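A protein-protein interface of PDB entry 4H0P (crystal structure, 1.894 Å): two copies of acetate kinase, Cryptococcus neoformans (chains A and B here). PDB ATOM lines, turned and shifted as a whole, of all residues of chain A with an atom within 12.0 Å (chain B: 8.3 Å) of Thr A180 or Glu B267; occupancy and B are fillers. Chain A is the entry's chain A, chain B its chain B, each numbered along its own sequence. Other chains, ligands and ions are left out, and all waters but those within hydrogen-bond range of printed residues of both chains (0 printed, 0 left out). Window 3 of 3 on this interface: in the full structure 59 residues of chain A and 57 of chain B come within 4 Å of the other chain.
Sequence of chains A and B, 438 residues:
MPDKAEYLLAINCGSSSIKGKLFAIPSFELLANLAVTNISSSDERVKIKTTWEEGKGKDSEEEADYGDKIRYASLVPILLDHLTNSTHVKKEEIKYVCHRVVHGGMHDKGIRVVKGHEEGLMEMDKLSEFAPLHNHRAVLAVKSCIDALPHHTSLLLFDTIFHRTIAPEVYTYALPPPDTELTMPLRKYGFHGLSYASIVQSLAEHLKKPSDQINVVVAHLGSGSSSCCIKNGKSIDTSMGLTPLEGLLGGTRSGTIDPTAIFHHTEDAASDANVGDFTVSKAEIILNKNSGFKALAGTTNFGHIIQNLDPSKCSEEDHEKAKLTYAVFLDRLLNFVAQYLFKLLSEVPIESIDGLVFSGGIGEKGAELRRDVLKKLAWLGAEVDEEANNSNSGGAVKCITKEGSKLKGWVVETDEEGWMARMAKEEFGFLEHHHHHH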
ATOM      1  N   GLU A 129      20.340  14.839  -8.428  1.00  0.00           N
ATOM      2  CA  GLU A 129      19.957  15.855  -7.448  1.00  0.00           C
ATOM      3  C   GLU A 129      18.616  15.554  -6.803  1.00  0.00           C
ATOM      4  O   GLU A 129      18.418  15.825  -5.626  1.00  0.00           O
ATOM      5  CB  GLU A 129      19.952  17.254  -8.083  1.00  0.00           C
ATOM      6  CG  GLU A 129      21.346  17.795  -8.364  1.00  0.00           C
ATOM      7  CD  GLU A 129      21.329  19.085  -9.182  1.00  0.00           C
ATOM      8  OE1 GLU A 129      20.496  19.973  -8.880  1.00  0.00           O
ATOM      9  OE2 GLU A 129      22.150  19.204 -10.127  1.00  0.00           O
ATOM     10  N   PHE A 130      17.699  14.989  -7.582  1.00  0.00           N
ATOM     11  CA  PHE A 130      16.386  14.652  -7.075  1.00  0.00           C
ATOM     12  C   PHE A 130      16.449  13.563  -6.003  1.00  0.00           C
ATOM     13  O   PHE A 130      15.776  13.654  -4.981  1.00  0.00           O
ATOM     14  CB  PHE A 130      15.442  14.202  -8.202  1.00  0.00           C
ATOM     15  CG  PHE A 130      14.043  13.965  -7.724  1.00  0.00           C
ATOM     16  CD1 PHE A 130      13.180  15.029  -7.530  1.00  0.00           C
ATOM     17  CD2 PHE A 130      13.608  12.685  -7.416  1.00  0.00           C
ATOM     18  CE1 PHE A 130      11.891  14.817  -7.057  1.00  0.00           C
ATOM     19  CE2 PHE A 130      12.326  12.464  -6.938  1.00  0.00           C
ATOM     20  CZ  PHE A 130      11.462  13.526  -6.758  1.00  0.00           C
ATOM     21  N   LEU A 175      -1.636  14.190  -3.467  1.00  0.00           N
ATOM     22  CA  LEU A 175      -1.013  15.369  -2.862  1.00  0.00           C
ATOM     23  C   LEU A 175      -1.299  16.577  -3.740  1.00  0.00           C
ATOM     24  O   LEU A 175      -1.467  16.432  -4.952  1.00  0.00           O
ATOM     25  CB  LEU A 175       0.507  15.181  -2.788  1.00  0.00           C
ATOM     26  CG  LEU A 175       1.091  14.103  -1.889  1.00  0.00           C
ATOM     27  CD1 LEU A 175       2.563  13.818  -2.226  1.00  0.00           C
ATOM     28  CD2 LEU A 175       0.945  14.557  -0.450  1.00  0.00           C
ATOM     29  N   PRO A 176      -1.349  17.776  -3.137  1.00  0.00           N
ATOM     30  CA  PRO A 176      -1.485  18.983  -3.966  1.00  0.00           C
ATOM     31  C   PRO A 176      -0.194  19.252  -4.736  1.00  0.00           C
ATOM     32  O   PRO A 176       0.802  18.563  -4.498  1.00  0.00           O
ATOM     33  CB  PRO A 176      -1.727  20.095  -2.937  1.00  0.00           C
ATOM     34  CG  PRO A 176      -1.126  19.584  -1.647  1.00  0.00           C
ATOM     35  CD  PRO A 176      -1.163  18.076  -1.704  1.00  0.00           C
ATOM     36  N   PRO A 177      -0.194  20.244  -5.653  1.00  0.00           N
ATOM     37  CA  PRO A 177       1.092  20.536  -6.313  1.00  0.00           C
ATOM     38  C   PRO A 177       2.178  20.942  -5.316  1.00  0.00           C
ATOM     39  O   PRO A 177       1.882  21.563  -4.286  1.00  0.00           O
ATOM     40  CB  PRO A 177       0.765  21.745  -7.201  1.00  0.00           C
ATOM     41  CG  PRO A 177      -0.683  21.619  -7.497  1.00  0.00           C
ATOM     42  CD  PRO A 177      -1.317  20.984  -6.264  1.00  0.00           C
ATOM     43  N   PRO A 178       3.436  20.599  -5.610  1.00  0.00           N
ATOM     44  CA  PRO A 178       4.498  21.011  -4.694  1.00  0.00           C
ATOM     45  C   PRO A 178       4.703  22.526  -4.698  1.00  0.00           C
ATOM     46  O   PRO A 178       4.237  23.207  -5.616  1.00  0.00           O
ATOM     47  CB  PRO A 178       5.739  20.297  -5.246  1.00  0.00           C
ATOM     48  CG  PRO A 178       5.393  19.921  -6.644  1.00  0.00           C
ATOM     49  CD  PRO A 178       3.921  19.685  -6.656  1.00  0.00           C
ATOM     50  N   ASP A 179       5.415  23.029  -3.691  1.00  0.00           N
ATOM     51  CA  ASP A 179       5.613  24.470  -3.506  1.00  0.00           C
ATOM     52  C   ASP A 179       6.467  25.093  -4.610  1.00  0.00           C
ATOM     53  O   ASP A 179       6.586  26.315  -4.702  1.00  0.00           O
ATOM     54  CB  ASP A 179       6.251  24.738  -2.130  1.00  0.00           C
ATOM     55  CG  ASP A 179       7.691  24.219  -2.023  1.00  0.00           C
ATOM     56  OD1 ASP A 179       8.196  23.562  -2.965  1.00  0.00           O
ATOM     57  OD2 ASP A 179       8.329  24.454  -0.972  1.00  0.00           O
ATOM     58  N   THR A 180       7.063  24.230  -5.428  1.00  0.00           N
ATOM     59  CA  THR A 180       8.053  24.614  -6.428  1.00  0.00           C
ATOM     60  C   THR A 180       8.004  23.588  -7.550  1.00  0.00           C
ATOM     61  O   THR A 180       7.607  22.448  -7.329  1.00  0.00           O
ATOM     62  CB  THR A 180       9.489  24.574  -5.834  1.00  0.00           C
ATOM     63  OG1 THR A 180       9.514  25.209  -4.544  1.00  0.00           O
ATOM     64  CG2 THR A 180      10.493  25.260  -6.765  1.00  0.00           C
ATOM     65  N   GLU A 181       8.416  23.982  -8.749  1.00  0.00           N
ATOM     66  CA  GLU A 181       8.552  23.045  -9.857  1.00  0.00           C
ATOM     67  C   GLU A 181       9.606  21.984  -9.549  1.00  0.00           C
ATOM     68  O   GLU A 181      10.776  22.310  -9.316  1.00  0.00           O
ATOM     69  CB  GLU A 181       8.959  23.798 -11.118  1.00  0.00           C
ATOM     70  CG  GLU A 181       9.189  22.916 -12.327  1.00  0.00           C
ATOM     71  CD  GLU A 181       8.014  22.932 -13.282  1.00  0.00           C
ATOM     72  OE1 GLU A 181       6.856  22.803 -12.811  1.00  0.00           O
ATOM     73  OE2 GLU A 181       8.256  23.088 -14.503  1.00  0.00           O
ATOM     74  N   LEU A 182       9.204  20.714  -9.548  1.00  0.00           N
ATOM     75  CA  LEU A 182      10.164  19.632  -9.318  1.00  0.00           C
ATOM     76  C   LEU A 182      10.605  18.967 -10.619  1.00  0.00           C
ATOM     77  O   LEU A 182       9.957  19.105 -11.654  1.00  0.00           O
ATOM     78  CB  LEU A 182       9.596  18.575  -8.365  1.00  0.00           C
ATOM     79  CG  LEU A 182       9.099  19.034  -7.001  1.00  0.00           C
ATOM     80  CD1 LEU A 182       8.574  17.846  -6.218  1.00  0.00           C
ATOM     81  CD2 LEU A 182      10.205  19.742  -6.228  1.00  0.00           C
ATOM     82  N   THR A 183      11.703  18.223 -10.533  1.00  0.00           N
ATOM     83  CA  THR A 183      12.292  17.499 -11.650  1.00  0.00           C
ATOM     84  C   THR A 183      11.348  16.439 -12.206  1.00  0.00           C
ATOM     85  O   THR A 183      11.356  16.139 -13.398  1.00  0.00           O
ATOM     86  CB  THR A 183      13.558  16.780 -11.170  1.00  0.00           C
ATOM     87  OG1 THR A 183      14.455  17.737 -10.589  1.00  0.00           O
ATOM     88  CG2 THR A 183      14.248  16.021 -12.317  1.00  0.00           C
ATOM     89  N   MET A 184      10.542  15.853 -11.330  1.00  0.00           N
ATOM     90  CA  MET A 184       9.620  14.816 -11.768  1.00  0.00           C
ATOM     91  C   MET A 184       8.447  14.841 -10.813  1.00  0.00           C
ATOM     92  O   MET A 184       8.558  15.365  -9.703  1.00  0.00           O
ATOM     93  CB  MET A 184      10.304  13.448 -11.729  1.00  0.00           C
ATOM     94  CG  MET A 184      10.676  13.005 -10.318  1.00  0.00           C
ATOM     95  SD  MET A 184      11.545  11.425 -10.172  1.00  0.00           S
ATOM     96  CE  MET A 184      13.118  11.864 -10.935  1.00  0.00           C
ATOM     97  N   PRO A 185       7.312  14.282 -11.238  1.00  0.00           N
ATOM     98  CA  PRO A 185       6.154  14.281 -10.335  1.00  0.00           C
ATOM     99  C   PRO A 185       6.363  13.432  -9.079  1.00  0.00           C
ATOM    100  O   PRO A 185       7.132  12.460  -9.102  1.00  0.00           O
ATOM    101  CB  PRO A 185       5.032  13.699 -11.206  1.00  0.00           C
ATOM    102  CG  PRO A 185       5.695  13.083 -12.388  1.00  0.00           C
ATOM    103  CD  PRO A 185       6.981  13.816 -12.596  1.00  0.00           C
ATOM    104  N   LEU A 186       5.675  13.778  -7.988  1.00  0.00           N
ATOM    105  CA  LEU A 186       5.688  12.937  -6.804  1.00  0.00           C
ATOM    106  C   LEU A 186       4.609  11.875  -6.988  1.00  0.00           C
ATOM    107  O   LEU A 186       3.412  12.180  -7.040  1.00  0.00           O
ATOM    108  CB  LEU A 186       5.418  13.778  -5.548  1.00  0.00           C
ATOM    109  CG  LEU A 186       6.408  14.928  -5.384  1.00  0.00           C
ATOM    110  CD1 LEU A 186       6.015  15.845  -4.220  1.00  0.00           C
ATOM    111  CD2 LEU A 186       7.812  14.351  -5.170  1.00  0.00           C
ATOM    112  N   LEU A 242       7.743   6.527  -4.179  1.00  0.00           N
ATOM    113  CA  LEU A 242       8.528   7.615  -4.725  1.00  0.00           C
ATOM    114  C   LEU A 242      10.017   7.265  -4.667  1.00  0.00           C
ATOM    115  O   LEU A 242      10.781   7.591  -5.576  1.00  0.00           O
ATOM    116  CB  LEU A 242       8.235   8.869  -3.922  1.00  0.00           C
ATOM    117  CG  LEU A 242       9.091  10.080  -4.266  1.00  0.00           C
ATOM    118  CD1 LEU A 242       8.824  10.501  -5.676  1.00  0.00           C
ATOM    119  CD2 LEU A 242       8.750  11.227  -3.304  1.00  0.00           C
ATOM    120  N   PHE A 263       8.570  13.195  12.310  1.00  0.00           N
ATOM    121  CA  PHE A 263       8.561  14.518  12.921  1.00  0.00           C
ATOM    122  C   PHE A 263       8.522  14.409  14.427  1.00  0.00           C
ATOM    123  O   PHE A 263       9.061  15.259  15.125  1.00  0.00           O
ATOM    124  CB  PHE A 263       7.415  15.347  12.361  1.00  0.00           C
ATOM    125  CG  PHE A 263       7.553  15.599  10.889  1.00  0.00           C
ATOM    126  CD1 PHE A 263       8.448  16.549  10.426  1.00  0.00           C
ATOM    127  CD2 PHE A 263       6.847  14.843   9.967  1.00  0.00           C
ATOM    128  CE1 PHE A 263       8.604  16.771   9.058  1.00  0.00           C
ATOM    129  CE2 PHE A 263       6.994  15.059   8.603  1.00  0.00           C
ATOM    130  CZ  PHE A 263       7.866  16.026   8.148  1.00  0.00           C
ATOM    131  N   ASP A 268      13.633  18.899  14.107  1.00  0.00           N
ATOM    132  CA  ASP A 268      14.187  19.524  12.903  1.00  0.00           C
ATOM    133  C   ASP A 268      14.454  18.488  11.816  1.00  0.00           C
ATOM    134  O   ASP A 268      15.523  18.461  11.201  1.00  0.00           O
ATOM    135  CB  ASP A 268      15.464  20.311  13.237  1.00  0.00           C
ATOM    136  CG  ASP A 268      15.208  21.433  14.225  1.00  0.00           C
ATOM    137  OD1 ASP A 268      14.203  22.151  14.046  1.00  0.00           O
ATOM    138  OD2 ASP A 268      15.997  21.581  15.187  1.00  0.00           O
ATOM    139  N   ALA A 269      13.463  17.638  11.586  1.00  0.00           N
ATOM    140  CA  ALA A 269      13.653  16.482  10.717  1.00  0.00           C
ATOM    141  C   ALA A 269      13.926  16.890   9.272  1.00  0.00           C
ATOM    142  O   ALA A 269      14.523  16.129   8.522  1.00  0.00           O
ATOM    143  CB  ALA A 269      12.444  15.546  10.807  1.00  0.00           C
ATOM    144  N   ALA A 270      13.473  18.085   8.880  1.00  0.00           N
ATOM    145  CA  ALA A 270      13.659  18.545   7.510  1.00  0.00           C
ATOM    146  C   ALA A 270      15.035  19.181   7.303  1.00  0.00           C
ATOM    147  O   ALA A 270      15.422  19.481   6.170  1.00  0.00           O
ATOM    148  CB  ALA A 270      12.573  19.520   7.117  1.00  0.00           C
ATOM    149  N   SER A 271      15.772  19.390   8.391  1.00  0.00           N
ATOM    150  CA  SER A 271      17.061  20.092   8.300  1.00  0.00           C
ATOM    151  C   SER A 271      18.138  19.219   7.679  1.00  0.00           C
ATOM    152  O   SER A 271      18.043  17.988   7.707  1.00  0.00           O
ATOM    153  CB  SER A 271      17.516  20.583   9.675  1.00  0.00           C
ATOM    154  OG  SER A 271      16.707  21.658  10.105  1.00  0.00           O
ATOM    155  N   ASP A 272      19.150  19.866   7.101  1.00  0.00           N
ATOM    156  CA  ASP A 272      20.260  19.170   6.456  1.00  0.00           C
ATOM    157  C   ASP A 272      20.982  18.283   7.456  1.00  0.00           C
ATOM    158  O   ASP A 272      21.206  18.672   8.603  1.00  0.00           O
ATOM    159  CB  ASP A 272      21.243  20.173   5.853  1.00  0.00           C
ATOM    160  CG  ASP A 272      20.632  20.986   4.725  1.00  0.00           C
ATOM    161  OD1 ASP A 272      19.391  20.938   4.540  1.00  0.00           O
ATOM    162  OD2 ASP A 272      21.403  21.681   4.023  1.00  0.00           O
ATOM    163  N   THR A 279      23.450  17.495   0.131  1.00  0.00           N
ATOM    164  CA  THR A 279      22.395  17.858   1.061  1.00  0.00           C
ATOM    165  C   THR A 279      21.287  16.789   1.075  1.00  0.00           C
ATOM    166  O   THR A 279      20.823  16.343   0.019  1.00  0.00           O
ATOM    167  CB  THR A 279      21.808  19.232   0.704  1.00  0.00           C
ATOM    168  OG1 THR A 279      22.831  20.235   0.821  1.00  0.00           O
ATOM    169  CG2 THR A 279      20.665  19.577   1.629  1.00  0.00           C
ATOM    170  N   VAL A 280      20.885  16.387   2.280  1.00  0.00           N
ATOM    171  CA  VAL A 280      19.846  15.375   2.487  1.00  0.00           C
ATOM    172  C   VAL A 280      19.264  15.578   3.891  1.00  0.00           C
ATOM    173  O   VAL A 280      20.006  15.870   4.825  1.00  0.00           O
ATOM    174  CB  VAL A 280      20.439  13.965   2.348  1.00  0.00           C
ATOM    175  CG1 VAL A 280      21.652  13.803   3.252  1.00  0.00           C
ATOM    176  CG2 VAL A 280      19.412  12.906   2.655  1.00  0.00           C
ATOM    177  N   SER A 281      17.946  15.460   4.051  1.00  0.00           N
ATOM    178  CA  SER A 281      17.348  15.724   5.364  1.00  0.00           C
ATOM    179  C   SER A 281      17.743  14.678   6.389  1.00  0.00           C
ATOM    180  O   SER A 281      18.079  13.536   6.041  1.00  0.00           O
ATOM    181  CB  SER A 281      15.829  15.782   5.294  1.00  0.00           C
ATOM    182  OG  SER A 281      15.310  14.525   4.908  1.00  0.00           O
ATOM    183  N   ALA A 283      15.733  13.358   8.376  1.00  0.00           N
ATOM    184  CA  ALA A 283      14.680  12.371   8.158  1.00  0.00           C
ATOM    185  C   ALA A 283      15.097  11.312   7.127  1.00  0.00           C
ATOM    186  O   ALA A 283      15.011  10.116   7.405  1.00  0.00           O
ATOM    187  CB  ALA A 283      13.394  13.058   7.735  1.00  0.00           C
ATOM    188  N   GLU A 284      15.574  11.716   5.949  1.00  0.00           N
ATOM    189  CA  GLU A 284      15.947  10.698   4.980  1.00  0.00           C
ATOM    190  C   GLU A 284      17.109   9.825   5.455  1.00  0.00           C
ATOM    191  O   GLU A 284      17.137   8.633   5.168  1.00  0.00           O
ATOM    192  CB  GLU A 284      16.256  11.298   3.617  1.00  0.00           C
ATOM    193  CG  GLU A 284      15.100  12.040   3.006  1.00  0.00           C
ATOM    194  CD  GLU A 284      15.528  12.885   1.820  1.00  0.00           C
ATOM    195  OE1 GLU A 284      15.908  12.296   0.776  1.00  0.00           O
ATOM    196  OE2 GLU A 284      15.495  14.133   1.949  1.00  0.00           O
ATOM    197  N   ILE B 262       7.057  14.280   1.440  1.00  0.00           N
ATOM    198  CA  ILE B 262       6.667  15.632   1.842  1.00  0.00           C
ATOM    199  C   ILE B 262       7.868  16.596   1.839  1.00  0.00           C
ATOM    200  O   ILE B 262       7.709  17.802   1.657  1.00  0.00           O
ATOM    201  CB  ILE B 262       5.984  15.622   3.216  1.00  0.00           C
ATOM    202  CG1 ILE B 262       5.302  16.968   3.518  1.00  0.00           C
ATOM    203  CG2 ILE B 262       6.983  15.255   4.299  1.00  0.00           C
ATOM    204  CD1 ILE B 262       4.142  17.332   2.597  1.00  0.00           C
ATOM    205  N   PHE B 263       9.063  16.044   2.006  1.00  0.00           N
ATOM    206  CA  PHE B 263      10.272  16.874   2.035  1.00  0.00           C
ATOM    207  C   PHE B 263      10.647  17.411   0.665  1.00  0.00           C
ATOM    208  O   PHE B 263      11.218  18.493   0.571  1.00  0.00           O
ATOM    209  CB  PHE B 263      11.451  16.112   2.634  1.00  0.00           C
ATOM    210  CG  PHE B 263      11.221  15.687   4.027  1.00  0.00           C
ATOM    211  CD1 PHE B 263      11.317  16.602   5.064  1.00  0.00           C
ATOM    212  CD2 PHE B 263      10.860  14.382   4.312  1.00  0.00           C
ATOM    213  CE1 PHE B 263      11.078  16.205   6.369  1.00  0.00           C
ATOM    214  CE2 PHE B 263      10.622  13.983   5.609  1.00  0.00           C
ATOM    215  CZ  PHE B 263      10.722  14.892   6.636  1.00  0.00           C
ATOM    216  N   HIS B 264      10.338  16.655  -0.390  1.00  0.00           N
ATOM    217  CA  HIS B 264      10.462  17.171  -1.758  1.00  0.00           C
ATOM    218  C   HIS B 264       9.334  18.159  -2.024  1.00  0.00           C
ATOM    219  O   HIS B 264       9.490  19.121  -2.745  1.00  0.00           O
ATOM    220  CB  HIS B 264      10.332  16.048  -2.801  1.00  0.00           C
ATOM    221  CG  HIS B 264      11.469  15.087  -2.822  1.00  0.00           C
ATOM    222  ND1 HIS B 264      11.478  13.930  -2.072  1.00  0.00           N
ATOM    223  CD2 HIS B 264      12.631  15.091  -3.524  1.00  0.00           C
ATOM    224  CE1 HIS B 264      12.597  13.266  -2.300  1.00  0.00           C
ATOM    225  NE2 HIS B 264      13.314  13.951  -3.180  1.00  0.00           N
ATOM    226  N   HIS B 265       8.172  17.889  -1.455  1.00  0.00           N
ATOM    227  CA  HIS B 265       6.979  18.627  -1.817  1.00  0.00           C
ATOM    228  C   HIS B 265       7.004  20.058  -1.288  1.00  0.00           C
ATOM    229  O   HIS B 265       6.504  20.990  -1.916  1.00  0.00           O
ATOM    230  CB  HIS B 265       5.759  17.882  -1.283  1.00  0.00           C
ATOM    231  CG  HIS B 265       4.467  18.550  -1.594  1.00  0.00           C
ATOM    232  ND1 HIS B 265       3.992  19.616  -0.868  1.00  0.00           N
ATOM    233  CD2 HIS B 265       3.536  18.287  -2.541  1.00  0.00           C
ATOM    234  CE1 HIS B 265       2.824  19.993  -1.363  1.00  0.00           C
ATOM    235  NE2 HIS B 265       2.531  19.209  -2.382  1.00  0.00           N
ATOM    236  N   THR B 266       7.577  20.216  -0.109  1.00  0.00           N
ATOM    237  CA  THR B 266       7.469  21.469   0.625  1.00  0.00           C
ATOM    238  C   THR B 266       8.774  21.751   1.367  1.00  0.00           C
ATOM    239  O   THR B 266       9.339  20.869   2.043  1.00  0.00           O
ATOM    240  CB  THR B 266       6.251  21.428   1.580  1.00  0.00           C
ATOM    241  OG1 THR B 266       5.056  21.746   0.845  1.00  0.00           O
ATOM    242  CG2 THR B 266       6.402  22.422   2.724  1.00  0.00           C
ATOM    243  N   GLU B 267       9.276  22.969   1.206  1.00  0.00           N
ATOM    244  CA  GLU B 267      10.486  23.375   1.903  1.00  0.00           C
ATOM    245  C   GLU B 267      10.197  23.541   3.403  1.00  0.00           C
ATOM    246  O   GLU B 267       9.084  23.908   3.796  1.00  0.00           O
ATOM    247  CB  GLU B 267      11.033  24.668   1.288  1.00  0.00           C
ATOM    248  CG  GLU B 267      11.752  24.444  -0.049  1.00  0.00           C
ATOM    249  CD  GLU B 267      11.522  25.559  -1.082  1.00  0.00           C
ATOM    250  OE1 GLU B 267      10.552  26.339  -0.939  1.00  0.00           O
ATOM    251  OE2 GLU B 267      12.315  25.642  -2.048  1.00  0.00           O
ATOM    252  N   ASP B 268      11.192  23.249   4.242  1.00  0.00           N
ATOM    253  CA  ASP B 268      11.051  23.433   5.689  1.00  0.00           C
ATOM    254  C   ASP B 268       9.796  22.738   6.220  1.00  0.00           C
ATOM    255  O   ASP B 268       9.050  23.320   7.002  1.00  0.00           O
ATOM    256  CB  ASP B 268      10.970  24.928   6.049  1.00  0.00           C
ATOM    257  CG  ASP B 268      11.897  25.793   5.211  1.00  0.00           C
ATOM    258  OD1 ASP B 268      13.102  25.474   5.124  1.00  0.00           O
ATOM    259  OD2 ASP B 268      11.410  26.795   4.635  1.00  0.00           O
ATOM    260  N   ALA B 269       9.562  21.505   5.783  1.00  0.00           N
ATOM    261  CA  ALA B 269       8.324  20.791   6.116  1.00  0.00           C
ATOM    262  C   ALA B 269       8.104  20.607   7.608  1.00  0.00           C
ATOM    263  O   ALA B 269       6.966  20.458   8.059  1.00  0.00           O
ATOM    264  CB  ALA B 269       8.299  19.431   5.418  1.00  0.00           C
ATOM    265  N   ALA B 270       9.193  20.566   8.371  1.00  0.00           N
ATOM    266  CA  ALA B 270       9.102  20.213   9.788  1.00  0.00           C
ATOM    267  C   ALA B 270       8.769  21.422  10.648  1.00  0.00           C
ATOM    268  O   ALA B 270       8.540  21.285  11.848  1.00  0.00           O
ATOM    269  CB  ALA B 270      10.386  19.544  10.268  1.00  0.00           C
ATOM    270  N   SER B 271       8.733  22.602  10.029  1.00  0.00           N
ATOM    271  CA  SER B 271       8.495  23.838  10.768  1.00  0.00           C
ATOM    272  C   SER B 271       7.034  24.053  11.107  1.00  0.00           C
ATOM    273  O   SER B 271       6.147  23.518  10.441  1.00  0.00           O
ATOM    274  CB  SER B 271       9.019  25.040   9.988  1.00  0.00           C
ATOM    275  OG  SER B 271      10.430  24.982   9.908  1.00  0.00           O
ATOM    276  N   LYS B 282       4.062  22.118   8.997  1.00  0.00           N
ATOM    277  CA  LYS B 282       3.456  22.343   7.696  1.00  0.00           C
ATOM    278  C   LYS B 282       3.170  20.988   7.056  1.00  0.00           C
ATOM    279  O   LYS B 282       2.176  20.832   6.352  1.00  0.00           O
ATOM    280  CB  LYS B 282       4.384  23.162   6.786  1.00  0.00           C
ATOM    281  CG  LYS B 282       4.516  24.630   7.160  1.00  0.00           C
ATOM    282  CD  LYS B 282       5.296  25.393   6.102  1.00  0.00           C
ATOM    283  CE  LYS B 282       6.694  24.832   5.961  1.00  0.00           C
ATOM    284  NZ  LYS B 282       7.546  25.554   4.955  1.00  0.00           N
ATOM    285  N   ALA B 283       4.051  20.022   7.310  1.00  0.00           N
ATOM    286  CA  ALA B 283       3.901  18.680   6.744  1.00  0.00           C
ATOM    287  C   ALA B 283       2.575  18.101   7.168  1.00  0.00           C
ATOM    288  O   ALA B 283       1.759  17.687   6.349  1.00  0.00           O
ATOM    289  CB  ALA B 283       5.016  17.777   7.196  1.00  0.00           C
ATOM    290  N   ILE B 286      -0.317  19.868   5.534  1.00  0.00           N
ATOM    291  CA  ILE B 286      -0.444  19.538   4.122  1.00  0.00           C
ATOM    292  C   ILE B 286      -1.030  18.134   3.943  1.00  0.00           C
ATOM    293  O   ILE B 286      -1.974  17.941   3.181  1.00  0.00           O
ATOM    294  CB  ILE B 286       0.899  19.676   3.406  1.00  0.00           C
ATOM    295  CG1 ILE B 286       1.260  21.159   3.287  1.00  0.00           C
ATOM    296  CG2 ILE B 286       0.853  19.057   2.012  1.00  0.00           C
ATOM    297  CD1 ILE B 286       2.696  21.384   2.916  1.00  0.00           C
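Of the 26 printed residues of chain A, 12 touch a printed residue of chain B.
Hydrophobic or aromatic side chains of chain A that line the printed part of chain B: Phe A130, Pro A176, Pro A178, Leu A182, Leu A186, Phe A263, Ala A270 and Ala A283.
Hydrophobic or aromatic side chains of chain B within 4 Å of the printed part of chain A: Phe B263, His B264, His B265, Ala B270 and Ala B283.
Among the printed residues, 19 pairs touch across the chains.
Among the printed residues, no Asp or Glu carboxylate lies within 4 Å of a Lys or Arg side-chain nitrogen of the other chain.
Phe A263 touches its own counterpart, Phe B263.
Phe A263 touches Ala B270, and with the chains exchanged Ala A270 touches Phe B263.
Ala A269 touches Ala B270, and with the chains exchanged Ala A270 touches Ala B269.
Ala B270 touches its own counterpart, Ala A270.
Of the 19 pairs that touch across the chains among the printed residues, 8 have their exchanged pair printed and touching as well.
Among the printed residues, merely in contact across the chains: Pro A178 with His B265, Asp A179 with Thr B266, Thr A180 with Glu B267, Leu A182 with His B264, Leu A186 with His B264, Leu A186 with His B265, Phe A263 with Phe B263, Phe A263 with Ala B270, Phe A263 with Ala B283, Ala A269 with Ala B270, Ala A270 with Phe B263, Ala A270 with Ala B269, Ala A270 with Ala B270 and Ala A283 with Phe B263.
O of Ala A269 sits at hydrogen-bond distance from N of Ala A283, 3.0 Å away.
A ring nitrogen (ND1) of His B265 is in hydrogen-bond range of the side-chain hydroxyl of Thr B266.
The backbone carbonyl oxygen (O) of Glu B267 is in hydrogen-bond range of the side-chain amino group (NZ) of Lys B282, 2.5 Å away.
O of Ala B269 is in hydrogen-bond range of N of Ala B283, at 3.0 Å.
Thr A180 touches just one residue of chain B: Glu B267.
Asp A179 touches three residues of chain B.
Of chain A, only Pro A176 (2.8 Å), Pro A177 (3.1 Å), Pro A178 (3.4 Å), Asp A179 (2.9 Å) and Leu A186 (3.6 Å) come within 4 Å of His B265.
Of chain A, only Asp A179 (3.5 Å) comes within 4 Å of Thr B266.
Of chain A, only Ala A270 comes within 4 Å of Ala B269.
Of the printed residues of chain B, Ala A269 touches Ala B270.
Printed residues of chain B within 4 Å of Pro A177: His B265 (3.1 Å).
Of the printed residues of chain B, Pro A176 touches His B265.
Lys B282 touches none of the printed residues of chain A.
Ser A271 touches none of the printed residues of chain B.
The nearest residue of chain B that does not touch Thr A180 is His B265 (4.8 Å).
The nearest residue of chain A that does not touch Glu B267 is Ala A270 (6.0 Å).
The backbone carbonyl oxygen of Phe A130 sits at hydrogen-bond distance from a ring nitrogen (NE2) of His B264, at 3.1 Å.
The backbone carbonyl oxygen of Pro A176 lies within hydrogen-bond range of a ring nitrogen (NE2) of His B265 (2.8 Å).
NE2 of His B265 sits at hydrogen-bond distance from O of Pro A177 (3.1 Å).
N of Asp A179 lies within hydrogen-bond range of O of His B265, at 2.9 Å.
The backbone NH (N) of Glu B267 is in hydrogen-bond range of the side-chain carboxylate (OD2) of Asp A179 (2.8 Å).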
